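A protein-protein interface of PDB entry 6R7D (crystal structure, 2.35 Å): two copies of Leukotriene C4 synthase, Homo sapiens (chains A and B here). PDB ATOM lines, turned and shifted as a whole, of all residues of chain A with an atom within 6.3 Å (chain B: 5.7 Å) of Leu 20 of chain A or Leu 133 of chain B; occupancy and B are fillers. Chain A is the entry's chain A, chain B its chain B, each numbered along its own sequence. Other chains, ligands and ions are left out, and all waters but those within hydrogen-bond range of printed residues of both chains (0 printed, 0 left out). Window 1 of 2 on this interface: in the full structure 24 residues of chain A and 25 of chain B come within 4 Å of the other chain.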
ATOM      1  N   VAL A  12      -5.540   8.608  14.056  1.00  0.00           N
ATOM      2  CA  VAL A  12      -5.566   7.466  14.957  1.00  0.00           C
ATOM      3  C   VAL A  12      -6.185   7.763  16.292  1.00  0.00           C
ATOM      4  O   VAL A  12      -6.105   6.935  17.221  1.00  0.00           O
ATOM      5  CB  VAL A  12      -4.119   6.886  15.120  1.00  0.00           C
ATOM      6  CG1 VAL A  12      -3.581   6.448  13.800  1.00  0.00           C
ATOM      7  CG2 VAL A  12      -3.154   7.824  15.743  1.00  0.00           C
ATOM      8  N   ALA A  13      -6.799   8.942  16.414  1.00  0.00           N
ATOM      9  CA  ALA A  13      -7.302   9.437  17.694  1.00  0.00           C
ATOM     10  C   ALA A  13      -8.460   8.595  18.178  1.00  0.00           C
ATOM     11  O   ALA A  13      -8.558   8.370  19.390  1.00  0.00           O
ATOM     12  CB  ALA A  13      -7.678  10.896  17.668  1.00  0.00           C
ATOM     13  N   LEU A  14      -9.274   8.106  17.268  1.00  0.00           N
ATOM     14  CA  LEU A  14     -10.374   7.242  17.679  1.00  0.00           C
ATOM     15  C   LEU A  14      -9.864   5.883  18.176  1.00  0.00           C
ATOM     16  O   LEU A  14     -10.367   5.368  19.168  1.00  0.00           O
ATOM     17  CB  LEU A  14     -11.403   7.031  16.552  1.00  0.00           C
ATOM     18  CG  LEU A  14     -12.027   8.306  15.918  1.00  0.00           C
ATOM     19  CD1 LEU A  14     -12.893   7.897  14.744  1.00  0.00           C
ATOM     20  CD2 LEU A  14     -12.928   8.995  16.908  1.00  0.00           C
ATOM     21  N   LEU A  15      -8.866   5.344  17.484  1.00  0.00           N
ATOM     22  CA  LEU A  15      -8.186   4.119  17.881  1.00  0.00           C
ATOM     23  C   LEU A  15      -7.594   4.333  19.283  1.00  0.00           C
ATOM     24  O   LEU A  15      -7.680   3.453  20.137  1.00  0.00           O
ATOM     25  CB  LEU A  15      -7.130   3.718  16.873  1.00  0.00           C
ATOM     26  CG  LEU A  15      -7.658   3.630  15.456  1.00  0.00           C
ATOM     27  CD1 LEU A  15      -6.518   3.214  14.534  1.00  0.00           C
ATOM     28  CD2 LEU A  15      -8.801   2.626  15.298  1.00  0.00           C
ATOM     29  N   ALA A  16      -6.995   5.494  19.510  1.00  0.00           N
ATOM     30  CA  ALA A  16      -6.317   5.742  20.766  1.00  0.00           C
ATOM     31  C   ALA A  16      -7.330   5.859  21.838  1.00  0.00           C
ATOM     32  O   ALA A  16      -7.077   5.408  22.994  1.00  0.00           O
ATOM     33  CB  ALA A  16      -5.453   7.008  20.629  1.00  0.00           C
ATOM     34  N   ALA A  17      -8.471   6.453  21.518  1.00  0.00           N
ATOM     35  CA  ALA A  17      -9.477   6.640  22.536  1.00  0.00           C
ATOM     36  C   ALA A  17     -10.080   5.285  22.944  1.00  0.00           C
ATOM     37  O   ALA A  17     -10.323   5.035  24.169  1.00  0.00           O
ATOM     38  CB  ALA A  17     -10.597   7.563  22.110  1.00  0.00           C
ATOM     39  N   VAL A  18     -10.377   4.455  21.961  1.00  0.00           N
ATOM     40  CA  VAL A  18     -10.881   3.108  22.234  1.00  0.00           C
ATOM     41  C   VAL A  18      -9.835   2.249  23.005  1.00  0.00           C
ATOM     42  O   VAL A  18     -10.179   1.549  23.966  1.00  0.00           O
ATOM     43  CB  VAL A  18     -11.303   2.434  20.953  1.00  0.00           C
ATOM     44  CG1 VAL A  18     -11.687   0.976  21.210  1.00  0.00           C
ATOM     45  CG2 VAL A  18     -12.519   3.134  20.386  1.00  0.00           C
ATOM     46  N   THR A  19      -8.558   2.366  22.626  1.00  0.00           N
ATOM     47  CA  THR A  19      -7.498   1.769  23.362  1.00  0.00           C
ATOM     48  C   THR A  19      -7.485   2.138  24.847  1.00  0.00           C
ATOM     49  O   THR A  19      -7.438   1.254  25.756  1.00  0.00           O
ATOM     50  CB  THR A  19      -6.165   2.174  22.739  1.00  0.00           C
ATOM     51  OG1 THR A  19      -6.128   1.661  21.419  1.00  0.00           O
ATOM     52  CG2 THR A  19      -4.936   1.621  23.585  1.00  0.00           C
ATOM     53  N   LEU A  20      -7.533   3.433  25.126  1.00  0.00           N
ATOM     54  CA  LEU A  20      -7.558   3.882  26.484  1.00  0.00           C
ATOM     55  C   LEU A  20      -8.815   3.426  27.275  1.00  0.00           C
ATOM     56  O   LEU A  20      -8.758   3.133  28.481  1.00  0.00           O
ATOM     57  CB  LEU A  20      -7.472   5.423  26.520  1.00  0.00           C
ATOM     58  CG  LEU A  20      -7.327   5.997  27.988  1.00  0.00           C
ATOM     59  CD1 LEU A  20      -6.037   5.564  28.637  1.00  0.00           C
ATOM     60  CD2 LEU A  20      -7.365   7.529  27.885  1.00  0.00           C
ATOM     61  N   LEU A  21      -9.955   3.502  26.617  1.00  0.00           N
ATOM     62  CA  LEU A  21     -11.176   2.940  27.164  1.00  0.00           C
ATOM     63  C   LEU A  21     -10.968   1.451  27.559  1.00  0.00           C
ATOM     64  O   LEU A  21     -11.387   1.045  28.645  1.00  0.00           O
ATOM     65  CB  LEU A  21     -12.359   3.144  26.233  1.00  0.00           C
ATOM     66  CG  LEU A  21     -13.737   2.777  26.834  1.00  0.00           C
ATOM     67  CD1 LEU A  21     -14.214   3.591  28.045  1.00  0.00           C
ATOM     68  CD2 LEU A  21     -14.761   2.971  25.726  1.00  0.00           C
ATOM     69  N   GLY A  22     -10.315   0.694  26.727  1.00  0.00           N
ATOM     70  CA  GLY A  22      -9.936  -0.636  27.021  1.00  0.00           C
ATOM     71  C   GLY A  22      -9.058  -0.751  28.272  1.00  0.00           C
ATOM     72  O   GLY A  22      -9.277  -1.668  29.093  1.00  0.00           O
ATOM     73  N   VAL A  23      -8.098   0.131  28.466  1.00  0.00           N
ATOM     74  CA  VAL A  23      -7.241   0.115  29.639  1.00  0.00           C
ATOM     75  C   VAL A  23      -8.089   0.370  30.879  1.00  0.00           C
ATOM     76  O   VAL A  23      -7.936  -0.306  31.892  1.00  0.00           O
ATOM     77  CB  VAL A  23      -6.093   1.126  29.512  1.00  0.00           C
ATOM     78  CG1 VAL A  23      -5.322   1.241  30.799  1.00  0.00           C
ATOM     79  CG2 VAL A  23      -5.186   0.670  28.427  1.00  0.00           C
ATOM     80  N   LEU A  24      -8.963   1.370  30.800  1.00  0.00           N
ATOM     81  CA  LEU A  24      -9.848   1.706  31.905  1.00  0.00           C
ATOM     82  C   LEU A  24     -10.798   0.550  32.295  1.00  0.00           C
ATOM     83  O   LEU A  24     -11.054   0.331  33.482  1.00  0.00           O
ATOM     84  CB  LEU A  24     -10.655   2.988  31.647  1.00  0.00           C
ATOM     85  CG  LEU A  24      -9.795   4.259  31.594  1.00  0.00           C
ATOM     86  CD1 LEU A  24     -10.586   5.473  30.953  1.00  0.00           C
ATOM     87  CD2 LEU A  24      -9.323   4.686  32.937  1.00  0.00           C
ATOM     88  N   LEU A  25     -11.289  -0.168  31.289  1.00  0.00           N
ATOM     89  CA  LEU A  25     -12.127  -1.268  31.520  1.00  0.00           C
ATOM     90  C   LEU A  25     -11.322  -2.383  32.297  1.00  0.00           C
ATOM     91  O   LEU A  25     -11.850  -2.997  33.214  1.00  0.00           O
ATOM     92  CB  LEU A  25     -12.688  -1.786  30.205  1.00  0.00           C
ATOM     93  CG  LEU A  25     -13.676  -2.979  30.364  1.00  0.00           C
ATOM     94  CD1 LEU A  25     -14.933  -2.525  31.151  1.00  0.00           C
ATOM     95  CD2 LEU A  25     -14.059  -3.577  29.012  1.00  0.00           C
ATOM     96  N   THR B  73      -0.763   2.599  27.148  1.00  0.00           N
ATOM     97  CA  THR B  73      -0.907   3.897  27.757  1.00  0.00           C
ATOM     98  C   THR B  73       0.370   4.706  27.559  1.00  0.00           C
ATOM     99  O   THR B  73       0.276   5.912  27.343  1.00  0.00           O
ATOM    100  CB  THR B  73      -1.271   3.861  29.272  1.00  0.00           C
ATOM    101  OG1 THR B  73      -0.123   3.246  29.908  1.00  0.00           O
ATOM    102  CG2 THR B  73      -2.374   2.945  29.513  1.00  0.00           C
ATOM    103  N   VAL B  76      -0.023   6.027  23.911  1.00  0.00           N
ATOM    104  CA  VAL B  76      -1.055   7.043  23.770  1.00  0.00           C
ATOM    105  C   VAL B  76      -0.639   8.322  24.452  1.00  0.00           C
ATOM    106  O   VAL B  76      -0.727   9.377  23.852  1.00  0.00           O
ATOM    107  CB  VAL B  76      -2.409   6.591  24.221  1.00  0.00           C
ATOM    108  CG1 VAL B  76      -3.405   7.708  24.198  1.00  0.00           C
ATOM    109  CG2 VAL B  76      -2.940   5.430  23.297  1.00  0.00           C
ATOM    110  N   PHE B  80      -0.082  11.825  22.227  1.00  0.00           N
ATOM    111  CA  PHE B  80      -1.072  12.843  22.439  1.00  0.00           C
ATOM    112  C   PHE B  80      -0.698  13.803  23.505  1.00  0.00           C
ATOM    113  O   PHE B  80      -1.299  14.862  23.581  1.00  0.00           O
ATOM    114  CB  PHE B  80      -2.455  12.257  22.704  1.00  0.00           C
ATOM    115  CG  PHE B  80      -3.045  11.653  21.511  1.00  0.00           C
ATOM    116  CD1 PHE B  80      -2.735  10.372  21.124  1.00  0.00           C
ATOM    117  CD2 PHE B  80      -3.829  12.441  20.614  1.00  0.00           C
ATOM    118  CE1 PHE B  80      -3.243   9.858  19.924  1.00  0.00           C
ATOM    119  CE2 PHE B  80      -4.321  11.901  19.401  1.00  0.00           C
ATOM    120  CZ  PHE B  80      -4.038  10.632  19.061  1.00  0.00           C
ATOM    121  N   VAL B 126      -2.120   6.923  32.480  1.00  0.00           N
ATOM    122  CA  VAL B 126      -3.521   7.015  32.093  1.00  0.00           C
ATOM    123  C   VAL B 126      -3.960   8.472  32.021  1.00  0.00           C
ATOM    124  O   VAL B 126      -4.663   8.856  31.073  1.00  0.00           O
ATOM    125  CB  VAL B 126      -4.427   6.189  32.979  1.00  0.00           C
ATOM    126  CG1 VAL B 126      -5.923   6.476  32.768  1.00  0.00           C
ATOM    127  CG2 VAL B 126      -4.129   4.671  32.800  1.00  0.00           C
ATOM    128  N   LEU B 128      -2.222  11.234  31.574  1.00  0.00           N
ATOM    129  CA  LEU B 128      -1.579  11.953  30.515  1.00  0.00           C
ATOM    130  C   LEU B 128      -2.202  11.572  29.177  1.00  0.00           C
ATOM    131  O   LEU B 128      -2.509  12.439  28.408  1.00  0.00           O
ATOM    132  CB  LEU B 128      -0.072  11.713  30.478  1.00  0.00           C
ATOM    133  CG  LEU B 128       0.684  12.163  31.698  1.00  0.00           C
ATOM    134  CD1 LEU B 128       2.163  11.915  31.450  1.00  0.00           C
ATOM    135  CD2 LEU B 128       0.468  13.604  32.117  1.00  0.00           C
ATOM    136  N   ALA B 129      -2.495  10.298  28.991  1.00  0.00           N
ATOM    137  CA  ALA B 129      -3.187   9.872  27.840  1.00  0.00           C
ATOM    138  C   ALA B 129      -4.554  10.485  27.745  1.00  0.00           C
ATOM    139  O   ALA B 129      -4.965  10.973  26.661  1.00  0.00           O
ATOM    140  CB  ALA B 129      -3.279   8.348  27.786  1.00  0.00           C
ATOM    141  N   ALA B 130      -5.279  10.478  28.846  1.00  0.00           N
ATOM    142  CA  ALA B 130      -6.616  11.071  28.844  1.00  0.00           C
ATOM    143  C   ALA B 130      -6.568  12.582  28.524  1.00  0.00           C
ATOM    144  O   ALA B 130      -7.420  13.051  27.792  1.00  0.00           O
ATOM    145  CB  ALA B 130      -7.359  10.851  30.176  1.00  0.00           C
ATOM    146  N   LEU B 131      -5.657  13.315  29.162  1.00  0.00           N
ATOM    147  CA  LEU B 131      -5.546  14.761  28.967  1.00  0.00           C
ATOM    148  C   LEU B 131      -5.233  15.044  27.506  1.00  0.00           C
ATOM    149  O   LEU B 131      -5.756  16.011  26.906  1.00  0.00           O
ATOM    150  CB  LEU B 131      -4.515  15.405  29.899  1.00  0.00           C
ATOM    151  CG  LEU B 131      -5.021  15.546  31.328  1.00  0.00           C
ATOM    152  CD1 LEU B 131      -3.868  15.819  32.287  1.00  0.00           C
ATOM    153  CD2 LEU B 131      -6.162  16.570  31.572  1.00  0.00           C
ATOM    154  N   GLY B 132      -4.362  14.222  26.942  1.00  0.00           N
ATOM    155  CA  GLY B 132      -3.927  14.375  25.531  1.00  0.00           C
ATOM    156  C   GLY B 132      -5.068  14.174  24.606  1.00  0.00           C
ATOM    157  O   GLY B 132      -5.300  14.958  23.688  1.00  0.00           O
ATOM    158  N   LEU B 133      -5.814  13.127  24.839  1.00  0.00           N
ATOM    159  CA  LEU B 133      -7.029  12.913  24.046  1.00  0.00           C
ATOM    160  C   LEU B 133      -8.108  13.996  24.219  1.00  0.00           C
ATOM    161  O   LEU B 133      -8.773  14.374  23.271  1.00  0.00           O
ATOM    162  CB  LEU B 133      -7.630  11.552  24.276  1.00  0.00           C
ATOM    163  CG  LEU B 133      -6.731  10.408  23.758  1.00  0.00           C
ATOM    164  CD1 LEU B 133      -7.243   9.062  24.332  1.00  0.00           C
ATOM    165  CD2 LEU B 133      -6.730  10.265  22.251  1.00  0.00           C
ATOM    166  N   LEU B 134      -8.290  14.475  25.446  1.00  0.00           N
ATOM    167  CA  LEU B 134      -9.179  15.614  25.692  1.00  0.00           C
ATOM    168  C   LEU B 134      -8.729  16.847  24.870  1.00  0.00           C
ATOM    169  O   LEU B 134      -9.552  17.457  24.276  1.00  0.00           O
ATOM    170  CB  LEU B 134      -9.216  15.977  27.200  1.00  0.00           C
ATOM    171  CG  LEU B 134     -10.506  15.818  28.063  1.00  0.00           C
ATOM    172  CD1 LEU B 134     -11.830  15.924  27.315  1.00  0.00           C
ATOM    173  CD2 LEU B 134     -10.485  14.446  28.757  1.00  0.00           C
ATOM    174  N   ALA B 135      -7.440  17.190  24.906  1.00  0.00           N
ATOM    175  CA  ALA B 135      -6.913  18.294  24.119  1.00  0.00           C
ATOM    176  C   ALA B 135      -7.157  18.083  22.616  1.00  0.00           C
ATOM    177  O   ALA B 135      -7.563  18.984  21.978  1.00  0.00           O
ATOM    178  CB  ALA B 135      -5.438  18.533  24.378  1.00  0.00           C
ATOM    179  N   HIS B 136      -7.127  16.865  22.136  1.00  0.00           N
ATOM    180  CA  HIS B 136      -7.392  16.593  20.758  1.00  0.00           C
ATOM    181  C   HIS B 136      -8.851  16.723  20.422  1.00  0.00           C
ATOM    182  O   HIS B 136      -9.164  17.260  19.425  1.00  0.00           O
ATOM    183  CB  HIS B 136      -6.874  15.223  20.354  1.00  0.00           C
ATOM    184  CG  HIS B 136      -7.215  14.868  18.948  1.00  0.00           C
ATOM    185  ND1 HIS B 136      -6.414  15.223  17.900  1.00  0.00           N
ATOM    186  CD2 HIS B 136      -8.261  14.219  18.407  1.00  0.00           C
ATOM    187  CE1 HIS B 136      -6.986  14.863  16.764  1.00  0.00           C
ATOM    188  NE2 HIS B 136      -8.124  14.292  17.041  1.00  0.00           N
ATOM    189  N   PHE B 137      -9.777  16.223  21.228  1.00  0.00           N
ATOM    190  CA  PHE B 137     -11.212  16.206  20.839  1.00  0.00           C
ATOM    191  C   PHE B 137     -12.073  17.337  21.385  1.00  0.00           C
ATOM    192  O   PHE B 137     -13.099  17.673  20.782  1.00  0.00           O
ATOM    193  CB  PHE B 137     -11.887  14.907  21.383  1.00  0.00           C
ATOM    194  CG  PHE B 137     -11.520  13.676  20.615  1.00  0.00           C
ATOM    195  CD1 PHE B 137     -11.961  13.503  19.296  1.00  0.00           C
ATOM    196  CD2 PHE B 137     -10.633  12.750  21.145  1.00  0.00           C
ATOM    197  CE1 PHE B 137     -11.629  12.368  18.560  1.00  0.00           C
ATOM    198  CE2 PHE B 137     -10.360  11.539  20.445  1.00  0.00           C
ATOM    199  CZ  PHE B 137     -10.835  11.366  19.148  1.00  0.00           C
ATOM    200  N   LEU B 138     -11.729  17.879  22.536  1.00  0.00           N
ATOM    201  CA  LEU B 138     -12.626  18.817  23.219  1.00  0.00           C
ATOM    202  C   LEU B 138     -12.879  20.114  22.429  1.00  0.00           C
ATOM    203  O   LEU B 138     -14.033  20.520  22.289  1.00  0.00           O
ATOM    204  CB  LEU B 138     -12.170  19.099  24.651  1.00  0.00           C
ATOM    205  CG  LEU B 138     -13.108  19.828  25.617  1.00  0.00           C
ATOM    206  CD1 LEU B 138     -14.426  19.035  25.803  1.00  0.00           C
ATOM    207  CD2 LEU B 138     -12.414  20.173  26.942  1.00  0.00           C
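Along chain A the printed residues that touch a printed residue of chain B span positions 13 to 24.
Of the 15 printed residues of chain B, 8 touch a printed residue of chain A.
Hydrophobic or aromatic side chains of chain B within 4 Å of the printed part of chain A: Val 76, Phe 80, Val 126, Leu 133, His 136 and Phe 137.
Among the printed residues, 13 pairs touch across the chains.
Among the printed residues, no Asp or Glu carboxylate lies within 4 Å of a Lys or Arg side-chain nitrogen of the other chain.
No position is printed for both chains.
Of the printed residues of chain B, Ala 13 of chain A touches Phe 80, Leu 133, His 136 and Phe 137.
Of the printed residues of chain B, Leu 20 of chain A touches Ala 130 and Leu 133.
Printed residues of chain B within 4 Å of Leu 24 of chain A: Val 126.
Leu 133 of chain B touches just these residues of chain A: Ala 13 (3.9 Å), Ala 16 (3.9 Å), Ala 17 (3.8 Å) and Leu 20 (3.9 Å).
The nearest printed residue of chain A that does not touch Val 76 of chain B is Thr 19 of chain A (4.3 Å).
Among the printed residues, pairs that only touch across the chains: Ala 13 of chain A with His 136 of chain B (3.5 Å), Ala 13 of chain A with Phe 137 of chain B (3.5 Å), Val 23 of chain A with Thr 73 of chain B (3.6 Å), Ala 16 of chain A with Phe 80 of chain B (3.7 Å), Ala 13 of chain A with Phe 80 of chain B (3.7 Å), Leu 20 of chain A with Ala 130 of chain B (3.7 Å), Ala 17 of chain A with Leu 133 of chain B (3.8 Å), Leu 24 of chain A with Val 126 of chain B (3.8 Å), Ala 16 of chain A with Leu 133 of chain B (3.9 Å), Leu 20 of chain A with Leu 133 of chain B (3.9 Å), Leu 14 of chain A with Phe 137 of chain B (3.9 Å), Ala 13 of chain A with Leu 133 of chain B (3.9 Å) and Ala 16 of chain A with Val 76 of chain B (3.99 Å).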
